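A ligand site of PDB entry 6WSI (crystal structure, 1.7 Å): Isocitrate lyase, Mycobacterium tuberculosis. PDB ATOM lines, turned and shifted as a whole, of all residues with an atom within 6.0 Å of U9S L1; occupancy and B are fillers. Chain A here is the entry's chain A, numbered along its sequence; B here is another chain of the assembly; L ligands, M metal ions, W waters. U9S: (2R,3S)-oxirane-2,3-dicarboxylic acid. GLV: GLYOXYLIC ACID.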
ATOM      1  N   TYR A  89     -24.458  10.029  -9.804  1.00  0.00           N
ATOM      2  CA  TYR A  89     -23.662   9.307  -8.808  1.00  0.00           C
ATOM      3  C   TYR A  89     -23.981   9.836  -7.417  1.00  0.00           C
ATOM      4  O   TYR A  89     -23.962  11.048  -7.179  1.00  0.00           O
ATOM      5  CB  TYR A  89     -22.155   9.413  -9.083  1.00  0.00           C
ATOM      6  CG  TYR A  89     -21.395   8.686  -8.002  1.00  0.00           C
ATOM      7  CD1 TYR A  89     -21.491   7.292  -7.877  1.00  0.00           C
ATOM      8  CD2 TYR A  89     -20.662   9.382  -7.039  1.00  0.00           C
ATOM      9  CE1 TYR A  89     -20.851   6.612  -6.855  1.00  0.00           C
ATOM     10  CE2 TYR A  89     -20.017   8.715  -6.014  1.00  0.00           C
ATOM     11  CZ  TYR A  89     -20.112   7.334  -5.925  1.00  0.00           C
ATOM     12  OH  TYR A  89     -19.472   6.675  -4.889  1.00  0.00           O
ATOM     13  N   SER A  91     -22.661   9.880  -3.818  1.00  0.00           N
ATOM     14  CA  SER A  91     -21.465   9.698  -3.011  1.00  0.00           C
ATOM     15  C   SER A  91     -21.770   9.583  -1.513  1.00  0.00           C
ATOM     16  O   SER A  91     -22.392  10.482  -0.939  1.00  0.00           O
ATOM     17  CB  SER A  91     -20.527  10.898  -3.239  1.00  0.00           C
ATOM     18  OG  SER A  91     -19.522  10.995  -2.241  1.00  0.00           O
ATOM     19  N   TRP A  93     -19.368   9.762   0.705  1.00  0.00           N
ATOM     20  CA  TRP A  93     -18.523  10.835   1.240  1.00  0.00           C
ATOM     21  C   TRP A  93     -19.310  12.142   1.355  1.00  0.00           C
ATOM     22  O   TRP A  93     -19.261  12.814   2.400  1.00  0.00           O
ATOM     23  CB  TRP A  93     -17.295  11.022   0.346  1.00  0.00           C
ATOM     24  CG  TRP A  93     -16.161  11.914   0.900  1.00  0.00           C
ATOM     25  CD1 TRP A  93     -14.907  11.497   1.270  1.00  0.00           C
ATOM     26  CD2 TRP A  93     -16.162  13.342   1.087  1.00  0.00           C
ATOM     27  NE1 TRP A  93     -14.155  12.556   1.707  1.00  0.00           N
ATOM     28  CE2 TRP A  93     -14.893  13.704   1.613  1.00  0.00           C
ATOM     29  CE3 TRP A  93     -17.115  14.350   0.883  1.00  0.00           C
ATOM     30  CZ2 TRP A  93     -14.557  15.014   1.935  1.00  0.00           C
ATOM     31  CZ3 TRP A  93     -16.779  15.669   1.201  1.00  0.00           C
ATOM     32  CH2 TRP A  93     -15.509  15.985   1.729  1.00  0.00           C
ATOM     33  N   ASP A 108     -15.366  10.623   6.113  1.00  0.00           N
ATOM     34  CA  ASP A 108     -15.912   9.489   5.359  1.00  0.00           C
ATOM     35  C   ASP A 108     -15.525   8.171   6.015  1.00  0.00           C
ATOM     36  O   ASP A 108     -14.652   7.432   5.545  1.00  0.00           O
ATOM     37  CB  ASP A 108     -15.443   9.575   3.911  1.00  0.00           C
ATOM     38  CG  ASP A 108     -16.123   8.578   2.997  1.00  0.00           C
ATOM     39  OD1 ASP A 108     -17.227   8.114   3.332  1.00  0.00           O
ATOM     40  OD2 ASP A 108     -15.530   8.245   1.934  1.00  0.00           O
ATOM     41  N   GLU A 182     -17.871  -2.287  -0.884  1.00  0.00           N
ATOM     42  CA  GLU A 182     -16.405  -2.318  -0.818  1.00  0.00           C
ATOM     43  C   GLU A 182     -15.930  -3.300   0.250  1.00  0.00           C
ATOM     44  O   GLU A 182     -16.619  -3.541   1.251  1.00  0.00           O
ATOM     45  CB  GLU A 182     -15.851  -0.928  -0.516  1.00  0.00           C
ATOM     46  CG  GLU A 182     -16.254  -0.399   0.854  1.00  0.00           C
ATOM     47  CD  GLU A 182     -16.335   1.123   0.908  1.00  0.00           C
ATOM     48  OE1 GLU A 182     -16.588   1.751  -0.153  1.00  0.00           O
ATOM     49  OE2 GLU A 182     -16.161   1.679   2.015  1.00  0.00           O
ATOM     50  N   LYS A 189     -14.279   1.832   8.398  1.00  0.00           N
ATOM     51  CA  LYS A 189     -14.370   2.239   6.996  1.00  0.00           C
ATOM     52  C   LYS A 189     -13.682   3.574   6.771  1.00  0.00           C
ATOM     53  O   LYS A 189     -13.761   4.472   7.610  1.00  0.00           O
ATOM     54  CB  LYS A 189     -15.837   2.335   6.551  1.00  0.00           C
ATOM     55  CG  LYS A 189     -16.061   2.786   5.086  1.00  0.00           C
ATOM     56  CD  LYS A 189     -16.245   4.313   4.943  1.00  0.00           C
ATOM     57  CE  LYS A 189     -16.745   4.730   3.550  1.00  0.00           C
ATOM     58  NZ  LYS A 189     -15.846   4.236   2.445  1.00  0.00           N
ATOM     59  N   LYS A 190     -13.018   3.707   5.620  1.00  0.00           N
ATOM     60  CA  LYS A 190     -12.394   4.960   5.210  1.00  0.00           C
ATOM     61  C   LYS A 190     -12.755   5.268   3.763  1.00  0.00           C
ATOM     62  O   LYS A 190     -13.017   4.369   2.972  1.00  0.00           O
ATOM     63  CB  LYS A 190     -10.866   4.904   5.313  1.00  0.00           C
ATOM     64  CG  LYS A 190     -10.355   4.452   6.670  1.00  0.00           C
ATOM     65  CD  LYS A 190     -10.650   5.498   7.719  1.00  0.00           C
ATOM     66  CE  LYS A 190      -9.816   5.266   8.977  1.00  0.00           C
ATOM     67  NZ  LYS A 190     -10.089   3.926   9.572  1.00  0.00           N
ATOM     68  N   CYS A 191     -12.740   6.551   3.428  1.00  0.00           N
ATOM     69  CA  CYS A 191     -12.585   6.934   2.030  1.00  0.00           C
ATOM     70  C   CYS A 191     -11.367   6.218   1.472  1.00  0.00           C
ATOM     71  O   CYS A 191     -10.377   6.019   2.175  1.00  0.00           O
ATOM     72  CB  CYS A 191     -12.426   8.462   1.930  1.00  0.00           C
ATOM     73  SG  CYS A 191     -11.797   9.084   0.355  1.00  0.00           S
ATOM     74  N   GLY A 192     -11.434   5.807   0.203  1.00  0.00           N
ATOM     75  CA  GLY A 192     -10.340   5.041  -0.362  1.00  0.00           C
ATOM     76  C   GLY A 192      -9.033   5.791  -0.415  1.00  0.00           C
ATOM     77  O   GLY A 192      -7.961   5.178  -0.538  1.00  0.00           O
ATOM     78  N   HIS A 193      -9.081   7.115  -0.317  1.00  0.00           N
ATOM     79  CA  HIS A 193      -7.888   7.945  -0.376  1.00  0.00           C
ATOM     80  C   HIS A 193      -7.502   8.489   0.993  1.00  0.00           C
ATOM     81  O   HIS A 193      -6.667   9.398   1.068  1.00  0.00           O
ATOM     82  CB  HIS A 193      -8.094   9.051  -1.415  1.00  0.00           C
ATOM     83  CG  HIS A 193      -8.431   8.496  -2.763  1.00  0.00           C
ATOM     84  ND1 HIS A 193      -9.673   8.662  -3.355  1.00  0.00           N
ATOM     85  CD2 HIS A 193      -7.713   7.720  -3.607  1.00  0.00           C
ATOM     86  CE1 HIS A 193      -9.686   8.036  -4.513  1.00  0.00           C
ATOM     87  NE2 HIS A 193      -8.517   7.465  -4.699  1.00  0.00           N
ATOM     88  N   ARG A 228     -16.320  -3.073  -5.243  1.00  0.00           N
ATOM     89  CA  ARG A 228     -15.146  -2.219  -5.100  1.00  0.00           C
ATOM     90  C   ARG A 228     -14.119  -2.892  -4.190  1.00  0.00           C
ATOM     91  O   ARG A 228     -14.477  -3.444  -3.149  1.00  0.00           O
ATOM     92  CB  ARG A 228     -15.540  -0.855  -4.538  1.00  0.00           C
ATOM     93  CG  ARG A 228     -14.408  -0.085  -3.880  1.00  0.00           C
ATOM     94  CD  ARG A 228     -14.880   1.242  -3.358  1.00  0.00           C
ATOM     95  NE  ARG A 228     -14.013   1.743  -2.289  1.00  0.00           N
ATOM     96  CZ  ARG A 228     -14.017   3.007  -1.877  1.00  0.00           C
ATOM     97  NH1 ARG A 228     -14.841   3.882  -2.452  1.00  0.00           N
ATOM     98  NH2 ARG A 228     -13.214   3.379  -0.899  1.00  0.00           N
ATOM     99  N   ASP A 230     -10.468  -2.237  -2.065  1.00  0.00           N
ATOM    100  CA  ASP A 230      -9.607  -1.215  -1.480  1.00  0.00           C
ATOM    101  C   ASP A 230      -8.192  -1.743  -1.225  1.00  0.00           C
ATOM    102  O   ASP A 230      -7.467  -1.177  -0.408  1.00  0.00           O
ATOM    103  CB  ASP A 230     -10.225  -0.698  -0.185  1.00  0.00           C
ATOM    104  CG  ASP A 230     -11.249   0.383  -0.425  1.00  0.00           C
ATOM    105  OD1 ASP A 230     -10.840   1.558  -0.533  1.00  0.00           O
ATOM    106  OD2 ASP A 230     -12.455   0.056  -0.526  1.00  0.00           O
ATOM    107  N   TRP A 283     -14.529  -2.320  -9.517  1.00  0.00           N
ATOM    108  CA  TRP A 283     -13.892  -1.012  -9.323  1.00  0.00           C
ATOM    109  C   TRP A 283     -12.723  -1.176  -8.359  1.00  0.00           C
ATOM    110  O   TRP A 283     -12.882  -1.707  -7.265  1.00  0.00           O
ATOM    111  CB  TRP A 283     -14.948  -0.016  -8.807  1.00  0.00           C
ATOM    112  CG  TRP A 283     -14.487   1.251  -8.107  1.00  0.00           C
ATOM    113  CD1 TRP A 283     -13.252   1.852  -8.170  1.00  0.00           C
ATOM    114  CD2 TRP A 283     -15.291   2.084  -7.267  1.00  0.00           C
ATOM    115  NE1 TRP A 283     -13.250   2.997  -7.389  1.00  0.00           N
ATOM    116  CE2 TRP A 283     -14.491   3.157  -6.826  1.00  0.00           C
ATOM    117  CE3 TRP A 283     -16.624   2.009  -6.831  1.00  0.00           C
ATOM    118  CZ2 TRP A 283     -14.977   4.161  -5.975  1.00  0.00           C
ATOM    119  CZ3 TRP A 283     -17.104   2.997  -5.985  1.00  0.00           C
ATOM    120  CH2 TRP A 283     -16.284   4.063  -5.575  1.00  0.00           C
ATOM    121  N   GLU A 285     -10.017   1.071  -6.324  1.00  0.00           N
ATOM    122  CA  GLU A 285      -9.531   2.382  -5.886  1.00  0.00           C
ATOM    123  C   GLU A 285      -8.037   2.494  -6.170  1.00  0.00           C
ATOM    124  O   GLU A 285      -7.305   1.520  -6.029  1.00  0.00           O
ATOM    125  CB  GLU A 285      -9.803   2.596  -4.394  1.00  0.00           C
ATOM    126  CG  GLU A 285     -11.238   2.976  -4.065  1.00  0.00           C
ATOM    127  CD  GLU A 285     -11.528   4.456  -4.319  1.00  0.00           C
ATOM    128  OE1 GLU A 285     -11.773   4.833  -5.493  1.00  0.00           O
ATOM    129  OE2 GLU A 285     -11.513   5.260  -3.365  1.00  0.00           O
ATOM    130  N   ASN A 313     -13.120   5.685 -10.491  1.00  0.00           N
ATOM    131  CA  ASN A 313     -13.320   6.908  -9.720  1.00  0.00           C
ATOM    132  C   ASN A 313     -12.330   7.971 -10.198  1.00  0.00           C
ATOM    133  O   ASN A 313     -11.138   7.881  -9.914  1.00  0.00           O
ATOM    134  CB  ASN A 313     -13.154   6.583  -8.227  1.00  0.00           C
ATOM    135  CG  ASN A 313     -13.159   7.809  -7.339  1.00  0.00           C
ATOM    136  OD1 ASN A 313     -13.466   8.908  -7.779  1.00  0.00           O
ATOM    137  ND2 ASN A 313     -12.820   7.618  -6.059  1.00  0.00           N
ATOM    138  N   CYS A 314     -12.827   8.983 -10.924  1.00  0.00           N
ATOM    139  CA  CYS A 314     -12.030  10.159 -11.284  1.00  0.00           C
ATOM    140  C   CYS A 314     -12.061  11.126 -10.113  1.00  0.00           C
ATOM    141  O   CYS A 314     -12.796  12.119 -10.097  1.00  0.00           O
ATOM    142  CB  CYS A 314     -12.572  10.808 -12.557  1.00  0.00           C
ATOM    143  SG  CYS A 314     -12.528   9.733 -14.041  1.00  0.00           S
ATOM    144  N   SER A 315     -11.218  10.868  -9.115  1.00  0.00           N
ATOM    145  CA  SER A 315     -11.427  11.409  -7.762  1.00  0.00           C
ATOM    146  C   SER A 315     -10.913  12.838  -7.658  1.00  0.00           C
ATOM    147  O   SER A 315      -9.805  13.133  -8.107  1.00  0.00           O
ATOM    148  CB  SER A 315     -10.720  10.525  -6.721  1.00  0.00           C
ATOM    149  OG  SER A 315     -10.654  11.170  -5.459  1.00  0.00           O
ATOM    150  N   PRO A 316     -11.685  13.747  -7.052  1.00  0.00           N
ATOM    151  CA  PRO A 316     -11.135  15.060  -6.648  1.00  0.00           C
ATOM    152  C   PRO A 316     -10.058  14.980  -5.573  1.00  0.00           C
ATOM    153  O   PRO A 316      -9.419  16.008  -5.278  1.00  0.00           O
ATOM    154  CB  PRO A 316     -12.365  15.815  -6.121  1.00  0.00           C
ATOM    155  CG  PRO A 316     -13.527  15.173  -6.858  1.00  0.00           C
ATOM    156  CD  PRO A 316     -13.156  13.720  -6.911  1.00  0.00           C
ATOM    157  N   SER A 317      -9.838  13.810  -4.966  1.00  0.00           N
ATOM    158  CA  SER A 317      -8.729  13.634  -4.041  1.00  0.00           C
ATOM    159  C   SER A 317      -7.386  13.601  -4.737  1.00  0.00           C
ATOM    160  O   SER A 317      -6.355  13.648  -4.057  1.00  0.00           O
ATOM    161  CB  SER A 317      -8.893  12.349  -3.213  1.00  0.00           C
ATOM    162  OG  SER A 317      -9.938  12.472  -2.262  1.00  0.00           O
ATOM    163  N   THR A 347     -16.570  11.615  -7.831  1.00  0.00           N
ATOM    164  CA  THR A 347     -17.260  11.409  -6.554  1.00  0.00           C
ATOM    165  C   THR A 347     -17.682  12.716  -5.879  1.00  0.00           C
ATOM    166  O   THR A 347     -18.854  12.892  -5.529  1.00  0.00           O
ATOM    167  CB  THR A 347     -16.362  10.613  -5.616  1.00  0.00           C
ATOM    168  OG1 THR A 347     -15.070  11.225  -5.587  1.00  0.00           O
ATOM    169  CG2 THR A 347     -16.243   9.153  -6.091  1.00  0.00           C
ATOM    170  N   LEU A 348     -16.728  13.623  -5.656  1.00  0.00           N
ATOM    171  CA  LEU A 348     -16.971  14.804  -4.823  1.00  0.00           C
ATOM    172  C   LEU A 348     -17.231  16.074  -5.642  1.00  0.00           C
ATOM    173  O   LEU A 348     -17.003  17.186  -5.150  1.00  0.00           O
ATOM    174  CB  LEU A 348     -15.809  15.026  -3.868  1.00  0.00           C
ATOM    175  CG  LEU A 348     -15.322  13.778  -3.103  1.00  0.00           C
ATOM    176  CD1 LEU A 348     -14.263  14.157  -2.054  1.00  0.00           C
ATOM    177  CD2 LEU A 348     -16.480  13.045  -2.466  1.00  0.00           C
ATOM    178  N   HIS B 393     -10.475  18.706   1.136  1.00  0.00           N
ATOM    179  CA  HIS B 393     -11.837  18.350   1.560  1.00  0.00           C
ATOM    180  C   HIS B 393     -11.851  17.443   2.793  1.00  0.00           C
ATOM    181  O   HIS B 393     -12.821  17.487   3.550  1.00  0.00           O
ATOM    182  CB  HIS B 393     -12.616  17.709   0.405  1.00  0.00           C
ATOM    183  CG  HIS B 393     -11.865  16.626  -0.325  1.00  0.00           C
ATOM    184  ND1 HIS B 393     -11.424  16.776  -1.619  1.00  0.00           N
ATOM    185  CD2 HIS B 393     -11.550  15.358   0.038  1.00  0.00           C
ATOM    186  CE1 HIS B 393     -10.833  15.661  -2.013  1.00  0.00           C
ATOM    187  NE2 HIS B 393     -10.894  14.788  -1.023  1.00  0.00           N
ATOM    188  N   GLN B 394     -10.805  16.642   3.025  1.00  0.00           N
ATOM    189  CA  GLN B 394     -10.820  15.728   4.172  1.00  0.00           C
ATOM    190  C   GLN B 394     -10.759  16.492   5.490  1.00  0.00           C
ATOM    191  O   GLN B 394     -11.578  16.253   6.400  1.00  0.00           O
ATOM    192  CB  GLN B 394      -9.670  14.714   4.110  1.00  0.00           C
ATOM    193  CG  GLN B 394      -9.470  14.013   2.747  1.00  0.00           C
ATOM    194  CD  GLN B 394     -10.555  12.984   2.425  1.00  0.00           C
ATOM    195  OE1 GLN B 394     -11.602  12.921   3.069  1.00  0.00           O
ATOM    196  NE2 GLN B 394     -10.306  12.173   1.391  1.00  0.00           N
ATOM    197  N   THR B 422      -4.093  10.623   0.461  1.00  0.00           N
ATOM    198  CA  THR B 422      -3.654  11.381  -0.702  1.00  0.00           C
ATOM    199  C   THR B 422      -3.762  12.887  -0.470  1.00  0.00           C
ATOM    200  O   THR B 422      -3.103  13.658  -1.185  1.00  0.00           O
ATOM    201  CB  THR B 422      -4.469  11.009  -1.959  1.00  0.00           C
ATOM    202  OG1 THR B 422      -5.835  11.400  -1.777  1.00  0.00           O
ATOM    203  CG2 THR B 422      -4.405   9.506  -2.223  1.00  0.00           C
HETATM  204  C02 U9S L   1     -12.731  10.308  -3.024  1.00  0.00           C
HETATM  205  C04 U9S L   1     -13.985  10.187  -2.158  1.00  0.00           C
HETATM  206  C05 U9S L   1     -14.422   8.886  -1.710  1.00  0.00           C
HETATM  207  C06 U9S L   1     -13.613   7.602  -1.993  1.00  0.00           C
HETATM  208  O01 U9S L   1     -11.599  10.357  -2.487  1.00  0.00           O
HETATM  209  O03 U9S L   1     -12.889  10.357  -4.280  1.00  0.00           O
HETATM  210  O07 U9S L   1     -12.789   7.525  -2.951  1.00  0.00           O
HETATM  211  O08 U9S L   1     -13.783   6.575  -1.263  1.00  0.00           O
HETATM  212  O09 U9S L   1     -15.051   9.532  -2.860  1.00  0.00           O
HETATM  213  C1  GLV L   2     -16.972   6.918  -2.866  1.00  0.00           C
HETATM  214  O1  GLV L   2     -17.160   5.872  -2.295  1.00  0.00           O
HETATM  215  C2  GLV L   2     -17.660   8.157  -2.281  1.00  0.00           C
HETATM  216  O2  GLV L   2     -17.798   9.223  -2.955  1.00  0.00           O
HETATM  217  O3  GLV L   2     -18.068   8.128  -1.094  1.00  0.00           O
HETATM  218 MG    MG M   1     -17.959   6.163  -0.413  1.00  0.00          MG
HETATM  219  O   HOH W   1     -15.980   6.241   0.367  1.00  0.00           O
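O01 of U9S L1 sits at hydrogen-bond distance from ND1 of His 193, at 2.7 Å.
N of Gly 192 sits at hydrogen-bond distance from O08 of U9S L1 (2.9 Å).
The side-chain hydroxyl of Ser 317 is in hydrogen-bond range of an oxygen (O01) of U9S L1, 2.7 Å away.
An oxygen (O03) of U9S L1 sits at hydrogen-bond distance from the side-chain hydroxyl (OG) of Ser 315 (2.7 Å).
The side-chain carboxylate of Glu 285 sits close to an oxygen (O07) of U9S L1.
An oxygen (O07) of U9S L1 is in hydrogen-bond range of the side-chain amide nitrogen of Asn 313 (3.1 Å).
SG of Cys 191 is in hydrogen-bond range of O01 of U9S L1 (3.1 Å).
O08 of U9S L1 is in salt-bridge range of NH1 of Arg 228, at 3.1 Å.
The backbone NH of Trp 93 sits close to an oxygen (O3) of GLV L2 (2.8 Å).
The side-chain hydroxyl of Ser 91 lies within hydrogen-bond range of an oxygen (O2) of GLV L2 (2.6 Å).
An oxygen (O03) of U9S L1 is in hydrogen-bond range of the side-chain hydroxyl (OG1) of Thr 347 (2.7 Å).
The guanidinium group of Arg 228 sits close to an oxygen (O1) of GLV L2, 3.1 Å away.
An oxygen (O09) of U9S L1 lies close to an oxygen (O2) of GLV L2 (2.8 Å).
OG of Ser 91 is in hydrogen-bond range of N of Trp 93.
The side-chain amide nitrogen (ND2) of Asn 313 is in hydrogen-bond range of the side-chain carboxylate (OE1) of Glu 285 (3.0 Å).
The guanidinium group (NE) of Arg 228 lies within salt-bridge range of the side-chain carboxylate (OD2) of Asp 230, 2.9 Å away.
The side-chain amide oxygen (OD1) of Asn 313 lies close to the backbone NH (N) of Ser 315, at 3.3 Å.
The side-chain hydroxyl of Ser 317 sits at hydrogen-bond distance from a ring nitrogen (NE2) of His 393 of chain B (2.8 Å).
OG of Ser 315 is in hydrogen-bond range of N of Ser 317, at 2.8 Å.
NE1 of Trp 93 is in hydrogen-bond range of OE1 of Gln 394 of chain B (2.9 Å).
The backbone carbonyl oxygen (O) of Ser 317 is in hydrogen-bond range of the side-chain hydroxyl (OG1) of Thr 422 of chain B (3.2 Å).
Trp 93 touches U9S L1.
Asp 108 touches U9S L1 (OD2 to C05, 3.9 Å).
CD2 of Leu 348 touches C04 of U9S L1 (3.8 Å).
Hydrophobic or aromatic side chains that line U9S L1: Trp 93, His 193 and Leu 348.
Within 4 Å of U9S L1: Trp 93, Asp 108, Cys 191, Gly 192, His 193, Arg 228, Glu 285, Asn 313, Ser 315, Ser 317, Thr 347 and Leu 348.
Water W1 lies within hydrogen-bond range of the side-chain carboxylate of Asp 108 (2.6 Å), an oxygen (O08) of U9S L1 (2.8 Å) and the side-chain amino group of Lys 189 (2.9 Å).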
